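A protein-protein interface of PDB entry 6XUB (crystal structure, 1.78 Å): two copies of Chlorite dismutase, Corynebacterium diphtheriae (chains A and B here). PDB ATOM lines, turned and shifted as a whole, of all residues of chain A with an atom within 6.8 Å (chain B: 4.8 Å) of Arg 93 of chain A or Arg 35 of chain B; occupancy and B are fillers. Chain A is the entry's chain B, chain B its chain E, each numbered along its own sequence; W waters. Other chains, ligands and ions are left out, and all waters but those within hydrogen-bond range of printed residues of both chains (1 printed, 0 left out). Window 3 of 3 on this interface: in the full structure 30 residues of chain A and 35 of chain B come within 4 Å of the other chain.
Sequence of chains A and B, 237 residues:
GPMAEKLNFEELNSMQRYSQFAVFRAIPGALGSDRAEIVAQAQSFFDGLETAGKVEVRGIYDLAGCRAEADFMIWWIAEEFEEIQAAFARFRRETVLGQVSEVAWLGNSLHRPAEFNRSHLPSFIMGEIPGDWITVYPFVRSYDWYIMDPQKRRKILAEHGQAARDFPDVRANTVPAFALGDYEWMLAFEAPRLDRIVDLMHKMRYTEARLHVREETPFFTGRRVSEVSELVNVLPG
O of Val 234 of chain B lies within hydrogen-bond range of NH1 of Arg 93 of chain A, 3.0 Å away.
The guanidinium group (NH1) of Arg 35 of chain B lies within hydrogen-bond range of the backbone carbonyl oxygen (O) of Leu 235 of chain B, 2.9 Å away.
The guanidinium group (NH1) of Arg 35 of chain B lies within hydrogen-bond range of the backbone carbonyl oxygen (O) of Val 232 of chain B, 2.7 Å away.
NE of Arg 35 of chain B is in hydrogen-bond range of O of Gly 32 of chain B (3.0 Å).
NH2 of Arg 35 of chain B is in hydrogen-bond range of O of Pro 236 of chain B (3.5 Å).
OE2 of Glu 94 of chain A lies within salt-bridge range of NH2 of Arg 93 of chain A (3.0 Å).
O of Gly 237 of chain B is in salt-bridge range of NH2 of Arg 35 of chain B (3.7 Å).
Among the printed residues, pairs that only touch across the chains: Arg 93 of chain A with Leu 235 of chain B (3.4 Å), Arg 93 of chain A with Asn 233 of chain B (3.5 Å), Ala 89 of chain A with Val 234 of chain B (3.5 Å), Arg 92 of chain A with Pro 236 of chain B (3.7 Å) and Arg 93 of chain A with Arg 35 of chain B (3.9 Å).
Gln 85 of chain A touches none of the printed residues of chain B.
Phe 91 of chain A touches none of the printed residues of chain B.
Of the printed residues of chain B, Arg 92 of chain A touches Pro 236.
Of chain B, only Arg 35, Asn 233, Val 234 and Leu 235 come within 4 Å of Arg 93 of chain A.
Of chain A, only Arg 93 comes within 4 Å of Arg 35 of chain B.
Printed residues of chain A within 4 Å of Val 234 of chain B: Ala 89 and Arg 93.
Of the printed residues of chain A, Pro 236 of chain B touches Arg 92.
The nearest residue of chain B that does not touch Arg 93 of chain A is Pro 236 of chain B (4.2 Å).
Of the 15 printed residues of chain B, 5 touch a printed residue of chain A.
Printed residues of chain B that touch a printed residue of chain A: Arg 35, Asn 233, Val 234, Leu 235 and Pro 236.
Hydrophobic or aromatic side chains of chain B that line the printed part of chain A: Val 234 and Pro 236.
Of the 13 printed residues of chain A, 3 touch a printed residue of chain B.
Hydrophobic or aromatic side chains of chain A that line the printed part of chain B: Ala 89.
Among the printed residues, 6 pairs touch across the chains.
No position is printed for both chains.
Water W1 lies within hydrogen-bond range of the backbone carbonyl oxygen of Ala 89 of chain A (2.7 Å) and the backbone carbonyl oxygen of Val 234 of chain B (2.8 Å).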
ATOM      1  N   GLN A  85      18.139   7.868   9.609  1.00  0.00           N
ATOM      2  CA  GLN A  85      17.314   9.001  10.007  1.00  0.00           C
ATOM      3  C   GLN A  85      16.906   9.817   8.796  1.00  0.00           C
ATOM      4  O   GLN A  85      15.731  10.197   8.639  1.00  0.00           O
ATOM      5  CB  GLN A  85      18.074   9.899  10.979  1.00  0.00           C
ATOM      6  CG  GLN A  85      18.201   9.430  12.358  1.00  0.00           C
ATOM      7  CD  GLN A  85      18.640  10.568  13.257  1.00  0.00           C
ATOM      8  OE1 GLN A  85      19.736  11.087  13.111  1.00  0.00           O
ATOM      9  NE2 GLN A  85      17.764  10.991  14.160  1.00  0.00           N
ATOM     10  N   ALA A  86      17.885  10.143   7.950  1.00  0.00           N
ATOM     11  CA  ALA A  86      17.620  10.964   6.782  1.00  0.00           C
ATOM     12  C   ALA A  86      16.661  10.265   5.837  1.00  0.00           C
ATOM     13  O   ALA A  86      15.749  10.890   5.287  1.00  0.00           O
ATOM     14  CB  ALA A  86      18.924  11.272   6.043  1.00  0.00           C
ATOM     15  N   PHE A  88      14.537   7.832   6.494  1.00  0.00           N
ATOM     16  CA  PHE A  88      13.220   7.772   7.133  1.00  0.00           C
ATOM     17  C   PHE A  88      12.500   9.104   6.998  1.00  0.00           C
ATOM     18  O   PHE A  88      11.350   9.164   6.547  1.00  0.00           O
ATOM     19  CB  PHE A  88      13.411   7.368   8.600  1.00  0.00           C
ATOM     20  CG  PHE A  88      12.152   7.431   9.462  1.00  0.00           C
ATOM     21  CD1 PHE A  88      11.273   6.353   9.533  1.00  0.00           C
ATOM     22  CD2 PHE A  88      11.889   8.541  10.242  1.00  0.00           C
ATOM     23  CE1 PHE A  88      10.127   6.407  10.325  1.00  0.00           C
ATOM     24  CE2 PHE A  88      10.760   8.588  11.057  1.00  0.00           C
ATOM     25  CZ  PHE A  88       9.877   7.515  11.098  1.00  0.00           C
ATOM     26  N   ALA A  89      13.167  10.191   7.366  1.00  0.00           N
ATOM     27  CA  ALA A  89      12.533  11.501   7.238  1.00  0.00           C
ATOM     28  C   ALA A  89      12.131  11.774   5.795  1.00  0.00           C
ATOM     29  O   ALA A  89      11.016  12.248   5.526  1.00  0.00           O
ATOM     30  CB  ALA A  89      13.470  12.584   7.775  1.00  0.00           C
ATOM     31  N   ARG A  90      13.001  11.427   4.838  1.00  0.00           N
ATOM     32  CA  ARG A  90      12.727  11.751   3.442  1.00  0.00           C
ATOM     33  C   ARG A  90      11.544  10.959   2.906  1.00  0.00           C
ATOM     34  O   ARG A  90      10.722  11.499   2.153  1.00  0.00           O
ATOM     35  CB  ARG A  90      14.009  11.508   2.617  1.00  0.00           C
ATOM     36  CG  ARG A  90      13.985  11.841   1.109  1.00  0.00           C
ATOM     37  CD  ARG A  90      15.481  11.906   0.511  1.00  0.00           C
ATOM     38  NE  ARG A  90      16.327  10.797   0.987  1.00  0.00           N
ATOM     39  CZ  ARG A  90      17.418  10.922   1.760  1.00  0.00           C
ATOM     40  NH1 ARG A  90      17.842  12.129   2.151  1.00  0.00           N
ATOM     41  NH2 ARG A  90      18.097   9.831   2.148  1.00  0.00           N
ATOM     42  N   PHE A  91      11.443   9.684   3.270  1.00  0.00           N
ATOM     43  CA  PHE A  91      10.278   8.884   2.917  1.00  0.00           C
ATOM     44  C   PHE A  91       8.997   9.557   3.391  1.00  0.00           C
ATOM     45  O   PHE A  91       8.048   9.725   2.618  1.00  0.00           O
ATOM     46  CB  PHE A  91      10.424   7.487   3.521  1.00  0.00           C
ATOM     47  CG  PHE A  91       9.238   6.572   3.272  1.00  0.00           C
ATOM     48  CD1 PHE A  91       9.044   5.980   2.028  1.00  0.00           C
ATOM     49  CD2 PHE A  91       8.351   6.284   4.295  1.00  0.00           C
ATOM     50  CE1 PHE A  91       7.978   5.134   1.808  1.00  0.00           C
ATOM     51  CE2 PHE A  91       7.279   5.451   4.086  1.00  0.00           C
ATOM     52  CZ  PHE A  91       7.102   4.861   2.844  1.00  0.00           C
ATOM     53  N   ARG A  92       8.974  10.001   4.648  1.00  0.00           N
ATOM     54  CA  ARG A  92       7.775  10.633   5.183  1.00  0.00           C
ATOM     55  C   ARG A  92       7.493  11.970   4.522  1.00  0.00           C
ATOM     56  O   ARG A  92       6.330  12.317   4.280  1.00  0.00           O
ATOM     57  CB  ARG A  92       7.908  10.838   6.685  1.00  0.00           C
ATOM     58  CG  ARG A  92       7.911   9.563   7.448  1.00  0.00           C
ATOM     59  CD  ARG A  92       8.053   9.835   8.906  1.00  0.00           C
ATOM     60  NE  ARG A  92       6.853  10.357   9.512  1.00  0.00           N
ATOM     61  CZ  ARG A  92       6.839  11.105  10.608  1.00  0.00           C
ATOM     62  NH1 ARG A  92       7.983  11.461  11.198  1.00  0.00           N
ATOM     63  NH2 ARG A  92       5.671  11.500  11.105  1.00  0.00           N
ATOM     64  N   ARG A  93       8.538  12.739   4.254  1.00  0.00           N
ATOM     65  CA  ARG A  93       8.404  14.117   3.830  1.00  0.00           C
ATOM     66  C   ARG A  93       8.231  14.227   2.326  1.00  0.00           C
ATOM     67  O   ARG A  93       7.474  15.079   1.860  1.00  0.00           O
ATOM     68  CB  ARG A  93       9.636  14.904   4.282  1.00  0.00           C
ATOM     69  CG  ARG A  93       9.622  16.391   3.960  1.00  0.00           C
ATOM     70  CD  ARG A  93      10.957  17.039   4.370  1.00  0.00           C
ATOM     71  NE  ARG A  93      12.067  16.542   3.560  1.00  0.00           N
ATOM     72  CZ  ARG A  93      13.023  15.704   3.978  1.00  0.00           C
ATOM     73  NH1 ARG A  93      13.036  15.255   5.225  1.00  0.00           N
ATOM     74  NH2 ARG A  93      13.987  15.320   3.136  1.00  0.00           N
ATOM     75  N   GLU A  94       8.898  13.371   1.555  1.00  0.00           N
ATOM     76  CA  GLU A  94       9.011  13.592   0.122  1.00  0.00           C
ATOM     77  C   GLU A  94       8.351  12.545  -0.774  1.00  0.00           C
ATOM     78  O   GLU A  94       8.473  12.652  -2.005  1.00  0.00           O
ATOM     79  CB  GLU A  94      10.504  13.718  -0.257  1.00  0.00           C
ATOM     80  CG  GLU A  94      11.188  14.960   0.317  1.00  0.00           C
ATOM     81  CD  GLU A  94      12.598  15.190  -0.242  1.00  0.00           C
ATOM     82  OE1 GLU A  94      13.002  14.502  -1.205  1.00  0.00           O
ATOM     83  OE2 GLU A  94      13.310  16.062   0.288  1.00  0.00           O
ATOM     84  N   THR A  95       7.650  11.552  -0.229  1.00  0.00           N
ATOM     85  CA  THR A  95       6.827  10.657  -1.047  1.00  0.00           C
ATOM     86  C   THR A  95       5.378  10.669  -0.575  1.00  0.00           C
ATOM     87  O   THR A  95       5.101  10.710   0.628  1.00  0.00           O
ATOM     88  CB  THR A  95       7.334   9.214  -1.024  1.00  0.00           C
ATOM     89  OG1 THR A  95       7.010   8.595   0.230  1.00  0.00           O
ATOM     90  CG2 THR A  95       8.848   9.172  -1.229  1.00  0.00           C
ATOM     91  N   VAL A  96       4.446  10.628  -1.525  1.00  0.00           N
ATOM     92  CA  VAL A  96       3.039  10.605  -1.146  1.00  0.00           C
ATOM     93  C   VAL A  96       2.745   9.372  -0.295  1.00  0.00           C
ATOM     94  O   VAL A  96       2.000   9.444   0.684  1.00  0.00           O
ATOM     95  CB  VAL A  96       2.154  10.685  -2.399  1.00  0.00           C
ATOM     96  CG1 VAL A  96       0.683  10.595  -2.027  1.00  0.00           C
ATOM     97  CG2 VAL A  96       2.401  11.994  -3.131  1.00  0.00           C
ATOM     98  N   GLY A  98       4.659   8.004   1.875  1.00  0.00           N
ATOM     99  CA  GLY A  98       5.038   8.349   3.232  1.00  0.00           C
ATOM    100  C   GLY A  98       4.131   9.396   3.838  1.00  0.00           C
ATOM    101  O   GLY A  98       3.941   9.435   5.062  1.00  0.00           O
ATOM    102  N   GLN A  99       3.544  10.241   2.996  1.00  0.00           N
ATOM    103  CA  GLN A  99       2.660  11.299   3.465  1.00  0.00           C
ATOM    104  C   GLN A  99       1.254  10.807   3.770  1.00  0.00           C
ATOM    105  O   GLN A  99       0.525  11.472   4.510  1.00  0.00           O
ATOM    106  CB  GLN A  99       2.570  12.416   2.420  1.00  0.00           C
ATOM    107  CG  GLN A  99       3.885  13.107   2.109  1.00  0.00           C
ATOM    108  CD  GLN A  99       3.839  13.872   0.797  1.00  0.00           C
ATOM    109  OE1 GLN A  99       2.855  13.807   0.072  1.00  0.00           O
ATOM    110  NE2 GLN A  99       4.904  14.602   0.490  1.00  0.00           N
ATOM    111  N   LEU B  31       2.487  21.804   8.648  1.00  0.00           N
ATOM    112  CA  LEU B  31       3.630  22.664   8.392  1.00  0.00           C
ATOM    113  C   LEU B  31       3.845  22.974   6.922  1.00  0.00           C
ATOM    114  O   LEU B  31       4.501  23.971   6.610  1.00  0.00           O
ATOM    115  CB  LEU B  31       4.896  22.006   8.965  1.00  0.00           C
ATOM    116  CG  LEU B  31       6.214  22.773   8.937  1.00  0.00           C
ATOM    117  CD1 LEU B  31       6.365  23.657  10.167  1.00  0.00           C
ATOM    118  CD2 LEU B  31       7.356  21.755   8.836  1.00  0.00           C
ATOM    119  N   GLY B  32       3.295  22.167   6.022  1.00  0.00           N
ATOM    120  CA  GLY B  32       3.441  22.441   4.615  1.00  0.00           C
ATOM    121  C   GLY B  32       4.911  22.388   4.239  1.00  0.00           C
ATOM    122  O   GLY B  32       5.749  21.825   4.943  1.00  0.00           O
ATOM    123  N   SER B  33       5.214  22.986   3.096  1.00  0.00           N
ATOM    124  CA  SER B  33       6.594  23.145   2.657  1.00  0.00           C
ATOM    125  C   SER B  33       6.872  24.613   2.336  1.00  0.00           C
ATOM    126  O   SER B  33       7.867  24.931   1.670  1.00  0.00           O
ATOM    127  CB  SER B  33       6.889  22.220   1.472  1.00  0.00           C
ATOM    128  OG  SER B  33       5.763  22.075   0.625  1.00  0.00           O
ATOM    129  N   ASP B  34       6.002  25.499   2.812  1.00  0.00           N
ATOM    130  CA  ASP B  34       6.312  26.910   2.996  1.00  0.00           C
ATOM    131  C   ASP B  34       6.872  27.135   4.404  1.00  0.00           C
ATOM    132  O   ASP B  34       6.269  27.753   5.268  1.00  0.00           O
ATOM    133  CB  ASP B  34       5.050  27.754   2.759  1.00  0.00           C
ATOM    134  CG  ASP B  34       5.355  29.131   2.254  1.00  0.00           C
ATOM    135  OD1 ASP B  34       4.558  30.034   2.556  1.00  0.00           O
ATOM    136  OD2 ASP B  34       6.374  29.317   1.540  1.00  0.00           O
ATOM    137  N   ARG B  35       8.061  26.598   4.608  1.00  0.00           N
ATOM    138  CA  ARG B  35       8.651  26.609   5.928  1.00  0.00           C
ATOM    139  C   ARG B  35       9.577  27.787   6.165  1.00  0.00           C
ATOM    140  O   ARG B  35      10.089  27.950   7.284  1.00  0.00           O
ATOM    141  CB  ARG B  35       9.452  25.327   6.148  1.00  0.00           C
ATOM    142  CG  ARG B  35       8.657  24.109   5.860  1.00  0.00           C
ATOM    143  CD  ARG B  35       9.536  22.893   5.721  1.00  0.00           C
ATOM    144  NE  ARG B  35       8.684  21.755   5.424  1.00  0.00           N
ATOM    145  CZ  ARG B  35       8.861  20.524   5.878  1.00  0.00           C
ATOM    146  NH1 ARG B  35       9.897  20.224   6.663  1.00  0.00           N
ATOM    147  NH2 ARG B  35       7.997  19.580   5.501  1.00  0.00           N
ATOM    148  N   ALA B  36       9.853  28.574   5.135  1.00  0.00           N
ATOM    149  CA  ALA B  36      10.882  29.593   5.273  1.00  0.00           C
ATOM    150  C   ALA B  36      10.489  30.608   6.336  1.00  0.00           C
ATOM    151  O   ALA B  36      11.288  30.939   7.224  1.00  0.00           O
ATOM    152  CB  ALA B  36      11.129  30.270   3.918  1.00  0.00           C
ATOM    153  N   GLU B  37       9.249  31.099   6.270  1.00  0.00           N
ATOM    154  CA  GLU B  37       8.756  32.012   7.294  1.00  0.00           C
ATOM    155  C   GLU B  37       8.739  31.351   8.670  1.00  0.00           C
ATOM    156  O   GLU B  37       9.043  31.996   9.678  1.00  0.00           O
ATOM    157  CB  GLU B  37       7.359  32.507   6.921  1.00  0.00           C
ATOM    158  CG  GLU B  37       7.317  33.945   6.428  1.00  0.00           C
ATOM    159  CD  GLU B  37       5.900  34.485   6.307  1.00  0.00           C
ATOM    160  OE1 GLU B  37       5.491  34.848   5.175  1.00  0.00           O
ATOM    161  OE2 GLU B  37       5.205  34.556   7.346  1.00  0.00           O
ATOM    162  N   ILE B  38       8.389  30.065   8.734  1.00  0.00           N
ATOM    163  CA  ILE B  38       8.288  29.393  10.029  1.00  0.00           C
ATOM    164  C   ILE B  38       9.667  29.274  10.666  1.00  0.00           C
ATOM    165  O   ILE B  38       9.844  29.557  11.857  1.00  0.00           O
ATOM    166  CB  ILE B  38       7.597  28.030   9.850  1.00  0.00           C
ATOM    167  CG1 ILE B  38       6.088  28.229   9.655  1.00  0.00           C
ATOM    168  CG2 ILE B  38       7.813  27.148  11.048  1.00  0.00           C
ATOM    169  CD1 ILE B  38       5.469  27.295   8.658  1.00  0.00           C
ATOM    170  N   VAL B  39      10.673  28.925   9.865  1.00  0.00           N
ATOM    171  CA  VAL B  39      12.037  28.810  10.359  1.00  0.00           C
ATOM    172  C   VAL B  39      12.517  30.149  10.892  1.00  0.00           C
ATOM    173  O   VAL B  39      13.057  30.239  11.998  1.00  0.00           O
ATOM    174  CB  VAL B  39      12.971  28.307   9.245  1.00  0.00           C
ATOM    175  CG1 VAL B  39      14.407  28.471   9.684  1.00  0.00           C
ATOM    176  CG2 VAL B  39      12.668  26.863   8.874  1.00  0.00           C
ATOM    177  N   VAL B 232      13.806  22.009  11.198  1.00  0.00           N
ATOM    178  CA  VAL B 232      12.519  22.228  10.556  1.00  0.00           C
ATOM    179  C   VAL B 232      12.495  21.628   9.154  1.00  0.00           C
ATOM    180  O   VAL B 232      11.455  21.142   8.697  1.00  0.00           O
ATOM    181  CB  VAL B 232      12.199  23.732  10.510  1.00  0.00           C
ATOM    182  CG1 VAL B 232      10.912  23.953   9.742  1.00  0.00           C
ATOM    183  CG2 VAL B 232      12.146  24.309  11.920  1.00  0.00           C
ATOM    184  N   ASN B 233      13.627  21.694   8.428  1.00  0.00           N
ATOM    185  CA  ASN B 233      13.685  21.165   7.065  1.00  0.00           C
ATOM    186  C   ASN B 233      13.578  19.643   7.001  1.00  0.00           C
ATOM    187  O   ASN B 233      13.232  19.106   5.947  1.00  0.00           O
ATOM    188  CB  ASN B 233      14.984  21.636   6.390  1.00  0.00           C
ATOM    189  CG  ASN B 233      14.992  23.124   6.144  1.00  0.00           C
ATOM    190  OD1 ASN B 233      13.932  23.765   6.114  1.00  0.00           O
ATOM    191  ND2 ASN B 233      16.184  23.695   5.971  1.00  0.00           N
ATOM    192  N   VAL B 234      13.862  18.942   8.096  1.00  0.00           N
ATOM    193  CA  VAL B 234      13.691  17.497   8.149  1.00  0.00           C
ATOM    194  C   VAL B 234      12.216  17.070   8.302  1.00  0.00           C
ATOM    195  O   VAL B 234      11.853  15.964   7.903  1.00  0.00           O
ATOM    196  CB  VAL B 234      14.530  16.956   9.327  1.00  0.00           C
ATOM    197  CG1 VAL B 234      14.268  15.480   9.560  1.00  0.00           C
ATOM    198  CG2 VAL B 234      16.000  17.202   9.085  1.00  0.00           C
ATOM    199  N   LEU B 235      11.360  17.906   8.877  1.00  0.00           N
ATOM    200  CA  LEU B 235      10.099  17.413   9.435  1.00  0.00           C
ATOM    201  C   LEU B 235       9.090  17.010   8.359  1.00  0.00           C
ATOM    202  O   LEU B 235       9.108  17.535   7.234  1.00  0.00           O
ATOM    203  CB  LEU B 235       9.475  18.481  10.329  1.00  0.00           C
ATOM    204  CG  LEU B 235      10.274  18.857  11.571  1.00  0.00           C
ATOM    205  CD1 LEU B 235       9.704  20.115  12.139  1.00  0.00           C
ATOM    206  CD2 LEU B 235      10.260  17.739  12.624  1.00  0.00           C
ATOM    207  N   PRO B 236       8.196  16.064   8.682  1.00  0.00           N
ATOM    208  CA  PRO B 236       7.217  15.611   7.675  1.00  0.00           C
ATOM    209  C   PRO B 236       6.319  16.729   7.209  1.00  0.00           C
ATOM    210  O   PRO B 236       5.983  16.800   6.024  1.00  0.00           O
ATOM    211  CB  PRO B 236       6.431  14.514   8.413  1.00  0.00           C
ATOM    212  CG  PRO B 236       6.560  14.863   9.829  1.00  0.00           C
ATOM    213  CD  PRO B 236       7.980  15.414   9.978  1.00  0.00           C
ATOM    214  N   GLY B 237       5.928  17.611   8.119  1.00  0.00           N
ATOM    215  CA  GLY B 237       5.163  18.790   7.772  1.00  0.00           C
ATOM    216  C   GLY B 237       4.170  18.612   6.643  1.00  0.00           C
ATOM    217  O   GLY B 237       4.313  19.251   5.602  1.00  0.00           O
ATOM    218  OXT GLY B 237       3.217  17.836   6.742  1.00  0.00           O
HETATM  219  O   HOH W   1      10.210  13.736   7.643  1.00  0.00           O
